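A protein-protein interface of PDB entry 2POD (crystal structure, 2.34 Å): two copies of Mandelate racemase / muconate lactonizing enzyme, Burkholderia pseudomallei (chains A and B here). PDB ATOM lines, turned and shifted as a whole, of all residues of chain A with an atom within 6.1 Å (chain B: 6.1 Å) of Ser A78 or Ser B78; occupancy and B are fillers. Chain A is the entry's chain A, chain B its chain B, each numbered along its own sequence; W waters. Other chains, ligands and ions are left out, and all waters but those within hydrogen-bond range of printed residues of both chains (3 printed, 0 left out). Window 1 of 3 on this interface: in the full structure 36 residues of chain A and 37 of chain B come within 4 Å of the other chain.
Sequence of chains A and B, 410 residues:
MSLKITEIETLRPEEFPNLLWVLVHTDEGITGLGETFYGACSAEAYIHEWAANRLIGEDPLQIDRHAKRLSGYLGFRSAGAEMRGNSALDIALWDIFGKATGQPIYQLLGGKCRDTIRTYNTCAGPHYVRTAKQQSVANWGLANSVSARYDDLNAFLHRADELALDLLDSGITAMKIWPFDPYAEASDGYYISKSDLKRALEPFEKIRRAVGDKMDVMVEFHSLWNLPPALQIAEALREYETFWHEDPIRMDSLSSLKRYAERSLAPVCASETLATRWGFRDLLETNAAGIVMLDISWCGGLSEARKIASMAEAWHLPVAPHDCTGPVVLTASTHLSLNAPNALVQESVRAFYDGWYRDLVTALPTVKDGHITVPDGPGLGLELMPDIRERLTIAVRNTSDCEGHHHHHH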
ATOM      1  N   LEU A  74       6.080  13.509   4.031  1.00  0.00           N
ATOM      2  CA  LEU A  74       5.789  12.077   3.966  1.00  0.00           C
ATOM      3  C   LEU A  74       4.287  11.848   3.946  1.00  0.00           C
ATOM      4  O   LEU A  74       3.524  12.638   4.506  1.00  0.00           O
ATOM      5  CB  LEU A  74       6.399  11.338   5.164  1.00  0.00           C
ATOM      6  CG  LEU A  74       7.921  11.332   5.366  1.00  0.00           C
ATOM      7  CD1 LEU A  74       8.254  10.739   6.716  1.00  0.00           C
ATOM      8  CD2 LEU A  74       8.625  10.560   4.255  1.00  0.00           C
ATOM      9  N   GLY A  75       3.862  10.770   3.293  1.00  0.00           N
ATOM     10  CA  GLY A  75       2.443  10.441   3.205  1.00  0.00           C
ATOM     11  C   GLY A  75       1.650  11.112   2.090  1.00  0.00           C
ATOM     12  O   GLY A  75       0.425  10.995   2.058  1.00  0.00           O
ATOM     13  N   PHE A  76       2.338  11.795   1.172  1.00  0.00           N
ATOM     14  CA  PHE A  76       1.692  12.499   0.048  1.00  0.00           C
ATOM     15  C   PHE A  76       1.150  11.595  -1.083  1.00  0.00           C
ATOM     16  O   PHE A  76       0.321  12.033  -1.891  1.00  0.00           O
ATOM     17  CB  PHE A  76       2.617  13.581  -0.535  1.00  0.00           C
ATOM     18  CG  PHE A  76       3.982  13.071  -0.926  1.00  0.00           C
ATOM     19  CD1 PHE A  76       5.060  13.191  -0.055  1.00  0.00           C
ATOM     20  CD2 PHE A  76       4.188  12.459  -2.162  1.00  0.00           C
ATOM     21  CE1 PHE A  76       6.311  12.707  -0.403  1.00  0.00           C
ATOM     22  CE2 PHE A  76       5.438  11.973  -2.515  1.00  0.00           C
ATOM     23  CZ  PHE A  76       6.503  12.099  -1.637  1.00  0.00           C
ATOM     24  N   ARG A  77       1.618  10.348  -1.143  1.00  0.00           N
ATOM     25  CA  ARG A  77       1.325   9.453  -2.273  1.00  0.00           C
ATOM     26  C   ARG A  77       0.161   8.492  -1.981  1.00  0.00           C
ATOM     27  O   ARG A  77      -0.162   7.619  -2.792  1.00  0.00           O
ATOM     28  CB  ARG A  77       2.590   8.684  -2.668  1.00  0.00           C
ATOM     29  CG  ARG A  77       2.748   8.295  -4.115  1.00  0.00           C
ATOM     30  CD  ARG A  77       4.096   7.637  -4.325  1.00  0.00           C
ATOM     31  NE  ARG A  77       4.162   6.969  -5.620  1.00  0.00           N
ATOM     32  CZ  ARG A  77       3.957   5.669  -5.797  1.00  0.00           C
ATOM     33  NH1 ARG A  77       4.037   5.147  -7.012  1.00  0.00           N
ATOM     34  NH2 ARG A  77       3.682   4.886  -4.759  1.00  0.00           N
ATOM     35  N   SER A  78      -0.483   8.669  -0.829  1.00  0.00           N
ATOM     36  CA  SER A  78      -1.620   7.828  -0.453  1.00  0.00           C
ATOM     37  C   SER A  78      -2.609   8.572   0.426  1.00  0.00           C
ATOM     38  O   SER A  78      -2.376   9.725   0.800  1.00  0.00           O
ATOM     39  CB  SER A  78      -1.139   6.588   0.298  1.00  0.00           C
ATOM     40  OG  SER A  78      -2.077   5.532   0.174  1.00  0.00           O
ATOM     41  N   ALA A  79      -3.695   7.881   0.770  1.00  0.00           N
ATOM     42  CA  ALA A  79      -4.767   8.420   1.604  1.00  0.00           C
ATOM     43  C   ALA A  79      -4.543   8.147   3.101  1.00  0.00           C
ATOM     44  O   ALA A  79      -5.457   7.714   3.806  1.00  0.00           O
ATOM     45  CB  ALA A  79      -6.115   7.842   1.152  1.00  0.00           C
ATOM     46  N   GLY A  80      -3.332   8.411   3.583  1.00  0.00           N
ATOM     47  CA  GLY A  80      -3.007   8.234   5.002  1.00  0.00           C
ATOM     48  C   GLY A  80      -3.589   9.319   5.895  1.00  0.00           C
ATOM     49  O   GLY A  80      -4.365  10.155   5.437  1.00  0.00           O
ATOM     50  N   MET A  83      -3.160  12.819   4.918  1.00  0.00           N
ATOM     51  CA  MET A  83      -3.979  13.140   3.748  1.00  0.00           C
ATOM     52  C   MET A  83      -5.448  13.350   4.105  1.00  0.00           C
ATOM     53  O   MET A  83      -6.098  14.230   3.551  1.00  0.00           O
ATOM     54  CB  MET A  83      -3.850  12.035   2.695  1.00  0.00           C
ATOM     55  CG  MET A  83      -4.595  12.296   1.388  1.00  0.00           C
ATOM     56  SD  MET A  83      -3.850  13.747   0.308  1.00  0.00           S
ATOM     57  CE  MET A  83      -2.009  13.133   0.173  1.00  0.00           C
ATOM     58  N   THR A 273      -9.260   4.745  -2.832  1.00  0.00           N
ATOM     59  CA  THR A 273      -8.040   4.576  -2.056  1.00  0.00           C
ATOM     60  C   THR A 273      -6.910   5.494  -2.567  1.00  0.00           C
ATOM     61  O   THR A 273      -5.855   5.606  -1.932  1.00  0.00           O
ATOM     62  CB  THR A 273      -7.567   3.116  -2.109  1.00  0.00           C
ATOM     63  OG1 THR A 273      -7.198   2.794  -3.456  1.00  0.00           O
ATOM     64  CG2 THR A 273      -8.671   2.174  -1.659  1.00  0.00           C
ATOM     65  N   LEU A 274      -7.138   6.135  -3.710  1.00  0.00           N
ATOM     66  CA  LEU A 274      -6.103   6.894  -4.419  1.00  0.00           C
ATOM     67  C   LEU A 274      -6.226   8.363  -4.018  1.00  0.00           C
ATOM     68  O   LEU A 274      -7.342   8.871  -3.847  1.00  0.00           O
ATOM     69  CB  LEU A 274      -6.314   6.754  -5.929  1.00  0.00           C
ATOM     70  CG  LEU A 274      -5.272   6.232  -6.929  1.00  0.00           C
ATOM     71  CD1 LEU A 274      -4.143   5.416  -6.327  1.00  0.00           C
ATOM     72  CD2 LEU A 274      -5.986   5.435  -7.992  1.00  0.00           C
ATOM     73  N   ALA A 275      -5.086   9.033  -3.868  1.00  0.00           N
ATOM     74  CA  ALA A 275      -5.062  10.434  -3.457  1.00  0.00           C
ATOM     75  C   ALA A 275      -4.373  11.353  -4.469  1.00  0.00           C
ATOM     76  O   ALA A 275      -3.357  10.988  -5.060  1.00  0.00           O
ATOM     77  CB  ALA A 275      -4.427  10.580  -2.062  1.00  0.00           C
ATOM     78  N   TRP A 298     -10.552  11.744   1.310  1.00  0.00           N
ATOM     79  CA  TRP A 298      -9.381  10.862   1.296  1.00  0.00           C
ATOM     80  C   TRP A 298      -8.350  11.297   0.271  1.00  0.00           C
ATOM     81  O   TRP A 298      -7.199  10.888   0.355  1.00  0.00           O
ATOM     82  CB  TRP A 298      -9.780   9.404   1.023  1.00  0.00           C
ATOM     83  CG  TRP A 298     -10.667   8.797   2.077  1.00  0.00           C
ATOM     84  CD1 TRP A 298     -10.854   9.244   3.360  1.00  0.00           C
ATOM     85  CD2 TRP A 298     -11.479   7.626   1.943  1.00  0.00           C
ATOM     86  NE1 TRP A 298     -11.739   8.436   4.020  1.00  0.00           N
ATOM     87  CE2 TRP A 298     -12.137   7.431   3.179  1.00  0.00           C
ATOM     88  CE3 TRP A 298     -11.715   6.722   0.902  1.00  0.00           C
ATOM     89  CZ2 TRP A 298     -13.014   6.374   3.399  1.00  0.00           C
ATOM     90  CZ3 TRP A 298     -12.599   5.670   1.122  1.00  0.00           C
ATOM     91  CH2 TRP A 298     -13.235   5.505   2.360  1.00  0.00           C
ATOM     92  N   LEU B  74      -6.370   2.063   3.832  1.00  0.00           N
ATOM     93  CA  LEU B  74      -5.938   3.361   3.302  1.00  0.00           C
ATOM     94  C   LEU B  74      -4.505   3.633   3.755  1.00  0.00           C
ATOM     95  O   LEU B  74      -4.060   3.106   4.777  1.00  0.00           O
ATOM     96  CB  LEU B  74      -6.850   4.466   3.828  1.00  0.00           C
ATOM     97  CG  LEU B  74      -8.007   5.094   3.037  1.00  0.00           C
ATOM     98  CD1 LEU B  74      -8.721   4.161   2.081  1.00  0.00           C
ATOM     99  CD2 LEU B  74      -9.002   5.728   3.993  1.00  0.00           C
ATOM    100  N   GLY B  75      -3.779   4.442   2.992  1.00  0.00           N
ATOM    101  CA  GLY B  75      -2.432   4.847   3.378  1.00  0.00           C
ATOM    102  C   GLY B  75      -1.335   3.833   3.107  1.00  0.00           C
ATOM    103  O   GLY B  75      -0.230   3.963   3.637  1.00  0.00           O
ATOM    104  N   PHE B  76      -1.624   2.832   2.276  1.00  0.00           N
ATOM    105  CA  PHE B  76      -0.641   1.795   1.928  1.00  0.00           C
ATOM    106  C   PHE B  76       0.386   2.204   0.853  1.00  0.00           C
ATOM    107  O   PHE B  76       1.370   1.491   0.613  1.00  0.00           O
ATOM    108  CB  PHE B  76      -1.336   0.488   1.535  1.00  0.00           C
ATOM    109  CG  PHE B  76      -2.410   0.660   0.496  1.00  0.00           C
ATOM    110  CD1 PHE B  76      -3.748   0.742   0.869  1.00  0.00           C
ATOM    111  CD2 PHE B  76      -2.087   0.736  -0.856  1.00  0.00           C
ATOM    112  CE1 PHE B  76      -4.738   0.917  -0.085  1.00  0.00           C
ATOM    113  CE2 PHE B  76      -3.077   0.910  -1.812  1.00  0.00           C
ATOM    114  CZ  PHE B  76      -4.402   0.993  -1.423  1.00  0.00           C
ATOM    115  N   ARG B  77       0.153   3.351   0.218  1.00  0.00           N
ATOM    116  CA  ARG B  77       0.873   3.728  -0.998  1.00  0.00           C
ATOM    117  C   ARG B  77       1.938   4.806  -0.771  1.00  0.00           C
ATOM    118  O   ARG B  77       2.593   5.207  -1.727  1.00  0.00           O
ATOM    119  CB  ARG B  77      -0.109   4.140  -2.105  1.00  0.00           C
ATOM    120  CG  ARG B  77       0.315   3.819  -3.537  1.00  0.00           C
ATOM    121  CD  ARG B  77      -0.798   4.163  -4.527  1.00  0.00           C
ATOM    122  NE  ARG B  77      -0.280   4.228  -5.890  1.00  0.00           N
ATOM    123  CZ  ARG B  77       0.176   5.336  -6.466  1.00  0.00           C
ATOM    124  NH1 ARG B  77       0.637   5.287  -7.703  1.00  0.00           N
ATOM    125  NH2 ARG B  77       0.162   6.495  -5.813  1.00  0.00           N
ATOM    126  N   SER B  78       2.092   5.273   0.478  1.00  0.00           N
ATOM    127  CA  SER B  78       3.362   5.866   0.932  1.00  0.00           C
ATOM    128  C   SER B  78       3.536   5.855   2.441  1.00  0.00           C
ATOM    129  O   SER B  78       2.930   5.027   3.126  1.00  0.00           O
ATOM    130  CB  SER B  78       3.583   7.282   0.390  1.00  0.00           C
ATOM    131  OG  SER B  78       2.602   8.176   0.860  1.00  0.00           O
ATOM    132  N   ALA B  79       4.391   6.756   2.933  1.00  0.00           N
ATOM    133  CA  ALA B  79       4.958   6.725   4.273  1.00  0.00           C
ATOM    134  C   ALA B  79       4.147   7.521   5.305  1.00  0.00           C
ATOM    135  O   ALA B  79       4.723   8.186   6.168  1.00  0.00           O
ATOM    136  CB  ALA B  79       6.393   7.242   4.221  1.00  0.00           C
ATOM    137  N   GLY B  80       2.821   7.434   5.232  1.00  0.00           N
ATOM    138  CA  GLY B  80       1.938   8.097   6.201  1.00  0.00           C
ATOM    139  C   GLY B  80       1.972   7.510   7.608  1.00  0.00           C
ATOM    140  O   GLY B  80       2.749   6.594   7.884  1.00  0.00           O
ATOM    141  N   MET B  83       1.761   3.826   7.955  1.00  0.00           N
ATOM    142  CA  MET B  83       2.975   3.170   7.458  1.00  0.00           C
ATOM    143  C   MET B  83       4.153   3.242   8.425  1.00  0.00           C
ATOM    144  O   MET B  83       4.894   2.274   8.572  1.00  0.00           O
ATOM    145  CB  MET B  83       3.384   3.766   6.106  1.00  0.00           C
ATOM    146  CG  MET B  83       4.533   3.058   5.412  1.00  0.00           C
ATOM    147  SD  MET B  83       4.184   1.206   4.900  1.00  0.00           S
ATOM    148  CE  MET B  83       2.437   1.374   4.054  1.00  0.00           C
ATOM    149  N   THR B 273      11.098   8.541   0.860  1.00  0.00           N
ATOM    150  CA  THR B 273       9.673   8.868   0.901  1.00  0.00           C
ATOM    151  C   THR B 273       8.778   7.720   0.429  1.00  0.00           C
ATOM    152  O   THR B 273       7.576   7.712   0.712  1.00  0.00           O
ATOM    153  CB  THR B 273       9.358  10.126   0.078  1.00  0.00           C
ATOM    154  OG1 THR B 273       9.506   9.838  -1.320  1.00  0.00           O
ATOM    155  CG2 THR B 273      10.291  11.270   0.466  1.00  0.00           C
ATOM    156  N   LEU B 274       9.365   6.766  -0.292  1.00  0.00           N
ATOM    157  CA  LEU B 274       8.611   5.671  -0.901  1.00  0.00           C
ATOM    158  C   LEU B 274       8.443   4.481   0.048  1.00  0.00           C
ATOM    159  O   LEU B 274       9.357   4.141   0.798  1.00  0.00           O
ATOM    160  CB  LEU B 274       9.285   5.215  -2.200  1.00  0.00           C
ATOM    161  CG  LEU B 274       9.090   6.089  -3.439  1.00  0.00           C
ATOM    162  CD1 LEU B 274      10.101   5.695  -4.502  1.00  0.00           C
ATOM    163  CD2 LEU B 274       7.655   5.986  -3.981  1.00  0.00           C
ATOM    164  N   ALA B 275       7.279   3.844  -0.003  1.00  0.00           N
ATOM    165  CA  ALA B 275       6.990   2.739   0.902  1.00  0.00           C
ATOM    166  C   ALA B 275       6.697   1.436   0.173  1.00  0.00           C
ATOM    167  O   ALA B 275       6.075   1.445  -0.882  1.00  0.00           O
ATOM    168  CB  ALA B 275       5.862   3.102   1.841  1.00  0.00           C
ATOM    169  N   TRP B 298      10.008   4.159   7.556  1.00  0.00           N
ATOM    170  CA  TRP B 298       9.025   4.821   6.694  1.00  0.00           C
ATOM    171  C   TRP B 298       8.489   3.911   5.599  1.00  0.00           C
ATOM    172  O   TRP B 298       7.488   4.247   4.973  1.00  0.00           O
ATOM    173  CB  TRP B 298       9.581   6.117   6.061  1.00  0.00           C
ATOM    174  CG  TRP B 298      10.055   7.160   7.040  1.00  0.00           C
ATOM    175  CD1 TRP B 298       9.690   7.290   8.352  1.00  0.00           C
ATOM    176  CD2 TRP B 298      10.982   8.222   6.779  1.00  0.00           C
ATOM    177  NE1 TRP B 298      10.339   8.357   8.924  1.00  0.00           N
ATOM    178  CE2 TRP B 298      11.135   8.950   7.981  1.00  0.00           C
ATOM    179  CE3 TRP B 298      11.699   8.631   5.647  1.00  0.00           C
ATOM    180  CZ2 TRP B 298      11.977  10.058   8.085  1.00  0.00           C
ATOM    181  CZ3 TRP B 298      12.542   9.738   5.752  1.00  0.00           C
ATOM    182  CH2 TRP B 298      12.672  10.436   6.963  1.00  0.00           C
HETATM  183  O   HOH W   1      -0.025   7.772   3.365  1.00  0.00           O
HETATM  184  O   HOH W   2      -2.475   7.764  -4.292  1.00  0.00           O
HETATM  185  O   HOH W   3       5.067   4.585  -1.884  1.00  0.00           O
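Leu A74 touches Thr B273, but with the chains exchanged Thr A273 does not touch Leu B74 (4.2 Å). Leu A74 touches Trp B298, and with the chains exchanged Trp A298 touches Leu B74. Gly A75 touches Gly B80, and with the chains exchanged Gly A80 touches Gly B75. Phe A76 touches Thr B273, and with the chains exchanged Thr A273 touches Phe B76. 12 positions are printed for both chains.
Of the printed residues of chain B, Ser A78 touches Gly B75, Phe B76, Arg B77 and Ser B78. Of the printed residues of chain B, Ala A79 touches Leu B74 (3.5 Å) and Gly B75 (3.8 Å). Printed residues of chain A within 4 Å of Ala B79: Leu A74 and Gly A75. Printed residues of chain A within 4 Å of Thr B273: Leu A74 (3.9 Å) and Phe A76 (3.8 Å). Of the printed residues of chain A, Leu B274 touches Arg A77. Ala B275 touches none of the printed residues of chain A. The nearest printed residue of chain A that does not touch Ser B78 is Leu A74 (5.1 Å).
Ala B79 touches Leu A74. CD2 of Leu A74 touches CA of Thr B273 (3.9 Å). CA of Gly A75 touches OG of Ser B78, 3.3 Å away. C of Ala B79 touches N of Gly A75, at 3.8 Å. OG1 of Thr B273 touches CZ of Phe A76, at 3.8 Å. Arg A77 touches Leu B274. Ser B78 touches Ser A78 (N to CB, 3.5 Å). Leu B74 touches Ala A79 (CB to O, 3.5 Å). Gly B75 touches Ala A79. Gly B75 touches Gly A80.
Hydrophobic or aromatic side chains of chain B that line the printed part of chain A: Leu B74, Phe B76, Ala B79, Leu B274 and Trp B298. Along chain B the printed residues that touch a printed residue of chain A span positions 74 to 298. Printed residues of chain A that touch a printed residue of chain B: Leu A74, Gly A75, Phe A76, Arg A77, Ser A78, Ala A79, Gly A80, Thr A273, Leu A274 and Trp A298. Hydrophobic or aromatic side chains of chain A within 4 Å of the printed part of chain B: Leu A74, Phe A76, Ala A79, Leu A274 and Trp A298. Among the printed residues, no Asp or Glu carboxylate lies within 4 Å of a Lys or Arg side-chain nitrogen of the other chain.
O of Arg B77 is in hydrogen-bond range of NH2 of Arg A77, 3.2 Å away. The side-chain hydroxyl (OG) of Ser B78 sits at hydrogen-bond distance from the backbone NH (N) of Arg A77 (3.1 Å). The backbone NH (N) of Gly B75 lies close to the side-chain hydroxyl (OG) of Ser A78 (3.5 Å). The backbone NH of Phe B76 is in hydrogen-bond range of the side-chain hydroxyl of Ser A78, 3.5 Å away. OG of Ser A78 is in hydrogen-bond range of N of Arg B77 (3.1 Å).
Water W3 lies within hydrogen-bond range of O of Arg B77, N of Ala B275 and NH2 of Arg A77. Water W2 lies within hydrogen-bond range of O of Arg A77 (2.8 Å), N of Ala A275 (2.9 Å) and NH2 of Arg B77 (3.3 Å). Water W1 lies within hydrogen-bond range of N of Gly A80 (3.4 Å) and N of Gly B80 (3.4 Å).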
